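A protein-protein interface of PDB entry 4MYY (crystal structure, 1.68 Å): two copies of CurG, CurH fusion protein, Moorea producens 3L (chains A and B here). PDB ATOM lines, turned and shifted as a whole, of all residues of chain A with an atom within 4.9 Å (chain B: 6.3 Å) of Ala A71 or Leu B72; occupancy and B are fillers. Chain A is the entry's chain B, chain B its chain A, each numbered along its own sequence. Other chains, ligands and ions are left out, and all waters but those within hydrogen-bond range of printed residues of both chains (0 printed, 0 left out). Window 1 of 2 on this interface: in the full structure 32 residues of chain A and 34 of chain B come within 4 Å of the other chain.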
ATOM      1  N   ILE A  24     -15.286  12.026  -1.812  1.00  0.00           N
ATOM      2  CA  ILE A  24     -14.726  10.987  -0.930  1.00  0.00           C
ATOM      3  C   ILE A  24     -13.623  10.203  -1.675  1.00  0.00           C
ATOM      4  O   ILE A  24     -12.551   9.931  -1.126  1.00  0.00           O
ATOM      5  CB  ILE A  24     -15.833  10.048  -0.382  1.00  0.00           C
ATOM      6  CG1 ILE A  24     -16.748  10.835   0.581  1.00  0.00           C
ATOM      7  CG2 ILE A  24     -15.236   8.818   0.297  1.00  0.00           C
ATOM      8  CD1 ILE A  24     -18.145  10.245   0.725  1.00  0.00           C
ATOM      9  N   ILE A  27     -10.507  12.210  -2.132  1.00  0.00           N
ATOM     10  CA  ILE A  27      -9.765  12.342  -0.876  1.00  0.00           C
ATOM     11  C   ILE A  27      -9.050  11.027  -0.605  1.00  0.00           C
ATOM     12  O   ILE A  27      -7.863  11.001  -0.272  1.00  0.00           O
ATOM     13  CB  ILE A  27     -10.646  12.844   0.306  1.00  0.00           C
ATOM     14  CG1 ILE A  27     -10.710  14.373   0.272  1.00  0.00           C
ATOM     15  CG2 ILE A  27     -10.021  12.506   1.653  1.00  0.00           C
ATOM     16  CD1 ILE A  27     -11.844  14.952  -0.532  1.00  0.00           C
ATOM     17  N   LEU A  28      -9.742   9.917  -0.803  1.00  0.00           N
ATOM     18  CA  LEU A  28      -9.111   8.628  -0.609  1.00  0.00           C
ATOM     19  C   LEU A  28      -7.871   8.428  -1.488  1.00  0.00           C
ATOM     20  O   LEU A  28      -6.833   7.973  -1.007  1.00  0.00           O
ATOM     21  CB  LEU A  28     -10.137   7.520  -0.854  1.00  0.00           C
ATOM     22  CG  LEU A  28      -9.794   6.168  -0.312  1.00  0.00           C
ATOM     23  CD1 LEU A  28      -9.380   6.193   1.159  1.00  0.00           C
ATOM     24  CD2 LEU A  28     -11.086   5.383  -0.482  1.00  0.00           C
ATOM     25  N   ILE A  31      -4.856  10.321  -0.204  1.00  0.00           N
ATOM     26  CA  ILE A  31      -4.269   9.574   0.907  1.00  0.00           C
ATOM     27  C   ILE A  31      -3.367   8.420   0.409  1.00  0.00           C
ATOM     28  O   ILE A  31      -2.208   8.294   0.825  1.00  0.00           O
ATOM     29  CB  ILE A  31      -5.394   9.077   1.869  1.00  0.00           C
ATOM     30  CG1 ILE A  31      -6.116  10.277   2.502  1.00  0.00           C
ATOM     31  CG2 ILE A  31      -4.828   8.167   2.937  1.00  0.00           C
ATOM     32  CD1 ILE A  31      -7.411   9.944   3.223  1.00  0.00           C
ATOM     33  N   ARG A  67     -15.880   2.813   1.101  1.00  0.00           N
ATOM     34  CA  ARG A  67     -14.813   3.800   0.805  1.00  0.00           C
ATOM     35  C   ARG A  67     -14.855   4.989   1.779  1.00  0.00           C
ATOM     36  O   ARG A  67     -13.821   5.452   2.229  1.00  0.00           O
ATOM     37  CB  ARG A  67     -14.868   4.284  -0.633  1.00  0.00           C
ATOM     38  CG  ARG A  67     -14.376   3.279  -1.679  1.00  0.00           C
ATOM     39  CD  ARG A  67     -14.251   3.948  -3.048  1.00  0.00           C
ATOM     40  NE  ARG A  67     -15.545   4.091  -3.703  1.00  0.00           N
ATOM     41  CZ  ARG A  67     -16.144   3.071  -4.319  1.00  0.00           C
ATOM     42  NH1 ARG A  67     -15.541   1.882  -4.369  1.00  0.00           N
ATOM     43  NH2 ARG A  67     -17.344   3.213  -4.853  1.00  0.00           N
ATOM     44  N   ALA A  68     -16.056   5.466   2.093  1.00  0.00           N
ATOM     45  CA  ALA A  68     -16.201   6.618   2.976  1.00  0.00           C
ATOM     46  C   ALA A  68     -15.694   6.243   4.360  1.00  0.00           C
ATOM     47  O   ALA A  68     -14.905   6.997   4.966  1.00  0.00           O
ATOM     48  CB  ALA A  68     -17.663   7.066   3.028  1.00  0.00           C
ATOM     49  N   ALA A  69     -16.128   5.073   4.842  1.00  0.00           N
ATOM     50  CA  ALA A  69     -15.724   4.622   6.160  1.00  0.00           C
ATOM     51  C   ALA A  69     -14.222   4.399   6.247  1.00  0.00           C
ATOM     52  O   ALA A  69     -13.625   4.703   7.299  1.00  0.00           O
ATOM     53  CB  ALA A  69     -16.504   3.389   6.600  1.00  0.00           C
ATOM     54  N   LEU A  70     -13.616   3.894   5.162  1.00  0.00           N
ATOM     55  CA  LEU A  70     -12.157   3.673   5.096  1.00  0.00           C
ATOM     56  C   LEU A  70     -11.402   5.001   5.210  1.00  0.00           C
ATOM     57  O   LEU A  70     -10.444   5.111   5.986  1.00  0.00           O
ATOM     58  CB  LEU A  70     -11.801   2.972   3.782  1.00  0.00           C
ATOM     59  CG  LEU A  70     -10.309   2.804   3.526  1.00  0.00           C
ATOM     60  CD1 LEU A  70      -9.711   1.866   4.571  1.00  0.00           C
ATOM     61  CD2 LEU A  70     -10.143   2.264   2.108  1.00  0.00           C
ATOM     62  N   ALA A  71     -11.819   6.001   4.431  1.00  0.00           N
ATOM     63  CA  ALA A  71     -11.227   7.341   4.526  1.00  0.00           C
ATOM     64  C   ALA A  71     -11.310   7.878   5.944  1.00  0.00           C
ATOM     65  O   ALA A  71     -10.332   8.446   6.427  1.00  0.00           O
ATOM     66  CB  ALA A  71     -11.937   8.305   3.590  1.00  0.00           C
ATOM     67  N   LEU A  72     -12.463   7.725   6.599  1.00  0.00           N
ATOM     68  CA  LEU A  72     -12.655   8.323   7.939  1.00  0.00           C
ATOM     69  C   LEU A  72     -11.750   7.631   8.918  1.00  0.00           C
ATOM     70  O   LEU A  72     -11.114   8.289   9.720  1.00  0.00           O
ATOM     71  CB  LEU A  72     -14.077   8.150   8.439  1.00  0.00           C
ATOM     72  CG  LEU A  72     -15.199   8.869   7.733  1.00  0.00           C
ATOM     73  CD1 LEU A  72     -16.487   8.572   8.491  1.00  0.00           C
ATOM     74  CD2 LEU A  72     -14.902  10.359   7.751  1.00  0.00           C
ATOM     75  N   LYS A  73     -11.716   6.304   8.856  1.00  0.00           N
ATOM     76  CA  LYS A  73     -10.826   5.545   9.741  1.00  0.00           C
ATOM     77  C   LYS A  73      -9.372   5.917   9.589  1.00  0.00           C
ATOM     78  O   LYS A  73      -8.645   6.031  10.568  1.00  0.00           O
ATOM     79  CB  LYS A  73     -10.984   4.056   9.499  1.00  0.00           C
ATOM     80  CG  LYS A  73     -11.909   3.430  10.485  1.00  0.00           C
ATOM     81  CD  LYS A  73     -11.125   3.208  11.762  1.00  0.00           C
ATOM     82  CE  LYS A  73     -11.823   2.208  12.642  1.00  0.00           C
ATOM     83  NZ  LYS A  73     -11.029   2.048  13.884  1.00  0.00           N
ATOM     84  N   LYS A  74      -8.936   6.067   8.351  1.00  0.00           N
ATOM     85  CA  LYS A  74      -7.583   6.455   8.074  1.00  0.00           C
ATOM     86  C   LYS A  74      -7.243   7.837   8.637  1.00  0.00           C
ATOM     87  O   LYS A  74      -6.195   8.016   9.258  1.00  0.00           O
ATOM     88  CB  LYS A  74      -7.333   6.420   6.573  1.00  0.00           C
ATOM     89  CG  LYS A  74      -5.996   6.985   6.173  1.00  0.00           C
ATOM     90  CD  LYS A  74      -4.822   6.184   6.733  1.00  0.00           C
ATOM     91  CE  LYS A  74      -3.513   6.920   6.455  1.00  0.00           C
ATOM     92  NZ  LYS A  74      -2.341   6.188   7.019  1.00  0.00           N
ATOM     93  N   LEU A  75      -8.120   8.811   8.419  1.00  0.00           N
ATOM     94  CA  LEU A  75      -7.852  10.156   8.954  1.00  0.00           C
ATOM     95  C   LEU A  75      -7.912  10.210  10.483  1.00  0.00           C
ATOM     96  O   LEU A  75      -7.187  10.979  11.119  1.00  0.00           O
ATOM     97  CB  LEU A  75      -8.828  11.157   8.363  1.00  0.00           C
ATOM     98  CG  LEU A  75      -8.698  11.426   6.855  1.00  0.00           C
ATOM     99  CD1 LEU A  75      -9.691  12.516   6.589  1.00  0.00           C
ATOM    100  CD2 LEU A  75      -7.310  11.839   6.390  1.00  0.00           C
ATOM    101  N   LEU B   4      -2.478   2.731   3.446  1.00  0.00           N
ATOM    102  CA  LEU B   4      -3.616   2.032   4.028  1.00  0.00           C
ATOM    103  C   LEU B   4      -3.184   0.644   4.428  1.00  0.00           C
ATOM    104  O   LEU B   4      -2.989  -0.223   3.571  1.00  0.00           O
ATOM    105  CB  LEU B   4      -4.784   1.916   3.053  1.00  0.00           C
ATOM    106  CG  LEU B   4      -5.457   3.233   2.721  1.00  0.00           C
ATOM    107  CD1 LEU B   4      -6.453   2.981   1.602  1.00  0.00           C
ATOM    108  CD2 LEU B   4      -6.119   3.855   3.949  1.00  0.00           C
ATOM    109  N   ILE B  31     -16.134  14.015  16.544  1.00  0.00           N
ATOM    110  CA  ILE B  31     -15.568  15.279  16.026  1.00  0.00           C
ATOM    111  C   ILE B  31     -16.472  16.477  16.337  1.00  0.00           C
ATOM    112  O   ILE B  31     -15.965  17.579  16.588  1.00  0.00           O
ATOM    113  CB  ILE B  31     -15.285  15.299  14.508  1.00  0.00           C
ATOM    114  CG1 ILE B  31     -14.836  13.965  13.982  1.00  0.00           C
ATOM    115  CG2 ILE B  31     -14.212  16.340  14.167  1.00  0.00           C
ATOM    116  CD1 ILE B  31     -15.407  13.707  12.611  1.00  0.00           C
ATOM    117  N   ARG B  67     -23.512  11.934   6.265  1.00  0.00           N
ATOM    118  CA  ARG B  67     -22.794  11.964   7.546  1.00  0.00           C
ATOM    119  C   ARG B  67     -21.285  11.708   7.329  1.00  0.00           C
ATOM    120  O   ARG B  67     -20.419  12.387   7.908  1.00  0.00           O
ATOM    121  CB  ARG B  67     -23.381  10.933   8.515  1.00  0.00           C
ATOM    122  CG  ARG B  67     -24.784  11.325   8.972  1.00  0.00           C
ATOM    123  CD  ARG B  67     -25.296  10.382  10.030  1.00  0.00           C
ATOM    124  NE  ARG B  67     -26.694  10.675  10.317  1.00  0.00           N
ATOM    125  CZ  ARG B  67     -27.515   9.830  10.921  1.00  0.00           C
ATOM    126  NH1 ARG B  67     -27.077   8.627  11.322  1.00  0.00           N
ATOM    127  NH2 ARG B  67     -28.784  10.191  11.138  1.00  0.00           N
ATOM    128  N   ALA B  68     -20.964  10.724   6.487  1.00  0.00           N
ATOM    129  CA  ALA B  68     -19.571  10.397   6.208  1.00  0.00           C
ATOM    130  C   ALA B  68     -18.843  11.574   5.546  1.00  0.00           C
ATOM    131  O   ALA B  68     -17.731  11.915   5.938  1.00  0.00           O
ATOM    132  CB  ALA B  68     -19.499   9.157   5.347  1.00  0.00           C
ATOM    133  N   ALA B  69     -19.497  12.222   4.585  1.00  0.00           N
ATOM    134  CA  ALA B  69     -18.878  13.360   3.918  1.00  0.00           C
ATOM    135  C   ALA B  69     -18.613  14.511   4.903  1.00  0.00           C
ATOM    136  O   ALA B  69     -17.545  15.134   4.872  1.00  0.00           O
ATOM    137  CB  ALA B  69     -19.756  13.831   2.798  1.00  0.00           C
ATOM    138  N   LEU B  70     -19.598  14.803   5.757  1.00  0.00           N
ATOM    139  CA  LEU B  70     -19.406  15.799   6.806  1.00  0.00           C
ATOM    140  C   LEU B  70     -18.275  15.447   7.728  1.00  0.00           C
ATOM    141  O   LEU B  70     -17.428  16.303   8.002  1.00  0.00           O
ATOM    142  CB  LEU B  70     -20.693  15.966   7.606  1.00  0.00           C
ATOM    143  CG  LEU B  70     -20.680  17.007   8.706  1.00  0.00           C
ATOM    144  CD1 LEU B  70     -20.418  18.418   8.164  1.00  0.00           C
ATOM    145  CD2 LEU B  70     -22.014  16.913   9.432  1.00  0.00           C
ATOM    146  N   ALA B  71     -18.249  14.202   8.201  1.00  0.00           N
ATOM    147  CA  ALA B  71     -17.168  13.750   9.095  1.00  0.00           C
ATOM    148  C   ALA B  71     -15.801  13.917   8.418  1.00  0.00           C
ATOM    149  O   ALA B  71     -14.830  14.352   9.051  1.00  0.00           O
ATOM    150  CB  ALA B  71     -17.401  12.307   9.504  1.00  0.00           C
ATOM    151  N   LEU B  72     -15.725  13.559   7.147  1.00  0.00           N
ATOM    152  CA  LEU B  72     -14.440  13.604   6.412  1.00  0.00           C
ATOM    153  C   LEU B  72     -13.936  15.032   6.276  1.00  0.00           C
ATOM    154  O   LEU B  72     -12.765  15.291   6.515  1.00  0.00           O
ATOM    155  CB  LEU B  72     -14.585  12.938   5.039  1.00  0.00           C
ATOM    156  CG  LEU B  72     -13.320  12.688   4.189  1.00  0.00           C
ATOM    157  CD1 LEU B  72     -12.278  11.933   4.980  1.00  0.00           C
ATOM    158  CD2 LEU B  72     -13.691  11.893   2.933  1.00  0.00           C
ATOM    159  N   LYS B  73     -14.827  15.961   5.945  1.00  0.00           N
ATOM    160  CA  LYS B  73     -14.474  17.377   5.893  1.00  0.00           C
ATOM    161  C   LYS B  73     -13.953  17.827   7.267  1.00  0.00           C
ATOM    162  O   LYS B  73     -12.902  18.466   7.376  1.00  0.00           O
ATOM    163  CB  LYS B  73     -15.664  18.232   5.422  1.00  0.00           C
ATOM    164  CG  LYS B  73     -15.260  19.671   5.066  1.00  0.00           C
ATOM    165  CD  LYS B  73     -15.057  20.489   6.328  1.00  0.00           C
ATOM    166  CE  LYS B  73     -14.682  21.933   6.049  1.00  0.00           C
ATOM    167  NZ  LYS B  73     -14.663  22.682   7.342  1.00  0.00           N
ATOM    168  N   LYS B  74     -14.682  17.467   8.319  1.00  0.00           N
ATOM    169  CA  LYS B  74     -14.319  17.923   9.647  1.00  0.00           C
ATOM    170  C   LYS B  74     -12.990  17.339  10.126  1.00  0.00           C
ATOM    171  O   LYS B  74     -12.194  18.049  10.736  1.00  0.00           O
ATOM    172  CB  LYS B  74     -15.453  17.656  10.628  1.00  0.00           C
ATOM    173  CG  LYS B  74     -16.681  18.538  10.367  1.00  0.00           C
ATOM    174  CD  LYS B  74     -17.708  18.384  11.464  1.00  0.00           C
ATOM    175  CE  LYS B  74     -17.306  19.239  12.667  1.00  0.00           C
ATOM    176  NZ  LYS B  74     -17.110  20.689  12.366  1.00  0.00           N
ATOM    177  N   LEU B  75     -12.753  16.060   9.841  1.00  0.00           N
ATOM    178  CA  LEU B  75     -11.450  15.439  10.174  1.00  0.00           C
ATOM    179  C   LEU B  75     -10.293  16.066   9.395  1.00  0.00           C
ATOM    180  O   LEU B  75      -9.229  16.351   9.964  1.00  0.00           O
ATOM    181  CB  LEU B  75     -11.494  13.931   9.913  1.00  0.00           C
ATOM    182  CG  LEU B  75     -12.346  13.171  10.907  1.00  0.00           C
ATOM    183  CD1 LEU B  75     -12.386  11.730  10.397  1.00  0.00           C
ATOM    184  CD2 LEU B  75     -11.729  13.206  12.286  1.00  0.00           C
ATOM    185  N   GLU B  76     -10.509  16.300   8.098  1.00  0.00           N
ATOM    186  CA  GLU B  76      -9.474  16.960   7.291  1.00  0.00           C
ATOM    187  C   GLU B  76      -9.165  18.350   7.772  1.00  0.00           C
ATOM    188  O   GLU B  76      -7.989  18.751   7.783  1.00  0.00           O
ATOM    189  CB  GLU B  76      -9.849  17.024   5.816  1.00  0.00           C
ATOM    190  CG  GLU B  76      -9.745  15.672   5.126  1.00  0.00           C
ATOM    191  CD  GLU B  76      -8.323  15.322   4.701  1.00  0.00           C
ATOM    192  OE1 GLU B  76      -7.345  15.705   5.390  1.00  0.00           O
ATOM    193  OE2 GLU B  76      -8.169  14.667   3.642  1.00  0.00           O
ATOM    194  N   THR B  77     -10.195  19.095   8.173  1.00  0.00           N
ATOM    195  CA  THR B  77      -9.982  20.444   8.676  1.00  0.00           C
ATOM    196  C   THR B  77      -9.160  20.387   9.950  1.00  0.00           C
ATOM    197  O   THR B  77      -8.219  21.170  10.152  1.00  0.00           O
ATOM    198  CB  THR B  77     -11.317  21.150   8.911  1.00  0.00           C
ATOM    199  OG1 THR B  77     -11.908  21.349   7.641  1.00  0.00           O
ATOM    200  CG2 THR B  77     -11.112  22.515   9.560  1.00  0.00           C
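Among the printed residues, pairs that only touch across the chains: Leu A75 with Leu B72 (3.1 Å), Leu A72 with Leu B72 (3.4 Å), Ile A27 with Glu B76 (3.5 Å), Leu A75 with Glu B76 (3.5 Å), Leu A72 with Ala B71 (3.6 Å), Ala A68 with Ala B68 (3.6 Å), Leu A72 with Ala B68 (3.7 Å), Leu A72 with Leu B75 (3.7 Å), Leu A70 with Leu B4 (3.8 Å), Lys A74 with Leu B4 (3.8 Å), Ala A71 with Leu B72 (3.9 Å), Ile A27 with Leu B72 (3.9 Å) and Ile A24 with Leu B72 (3.9996 Å).
Ile A31 touches none of the printed residues of chain B.
Ala A71 touches one residue of chain B.
Of the printed residues of chain B, Leu A75 touches Leu B72 and Glu B76.
Of the printed residues of chain A, Leu B4 touches Leu A70 (3.8 Å) and Lys A74 (3.8 Å).
Of the printed residues of chain A, Ala B68 touches Ala A68 (3.6 Å) and Leu A72 (3.7 Å).
Printed residues of chain A within 4 Å of Leu B72: Ile A24 (3.9996 Å), Ile A27 (3.9 Å), Ala A71 (3.9 Å), Leu A72 (3.4 Å) and Leu A75 (3.1 Å).
Lys B73 touches none of the printed residues of chain A.
The nearest residue of chain B that does not touch Ala A71 is Leu B75 (5.5 Å).
The nearest printed residue of chain A that does not touch Leu B72 is Ala A68 (5.4 Å).
Hydrophobic or aromatic side chains of chain A within 4 Å of the printed part of chain B: Ile A24, Ile A27, Ala A68, Leu A70, Ala A71, Leu A72 and Leu A75.
Of the 13 printed residues of chain B, 6 touch a printed residue of chain A.
Printed residues of chain B that touch a printed residue of chain A: Leu B4, Ala B68, Ala B71, Leu B72, Leu B75 and Glu B76.
Hydrophobic or aromatic side chains of chain B within 4 Å of the printed part of chain A: Leu B4, Ala B68, Ala B71, Leu B72 and Leu B75.
Among the printed residues, no Asp or Glu carboxylate lies within 4 Å of a Lys or Arg side-chain nitrogen of the other chain.
Ala B68 touches its own counterpart, Ala A68.
Leu A72 touches Ala B68, but with the chains exchanged Ala A68 does not touch Leu B72 (5.4 Å).
Leu B72 touches its own counterpart, Leu A72.
Leu A72 touches Leu B75, and with the chains exchanged Leu A75 touches Leu B72.
Of the 13 pairs that touch across the chains among the printed residues, 6 have their exchanged pair printed and touching as well.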
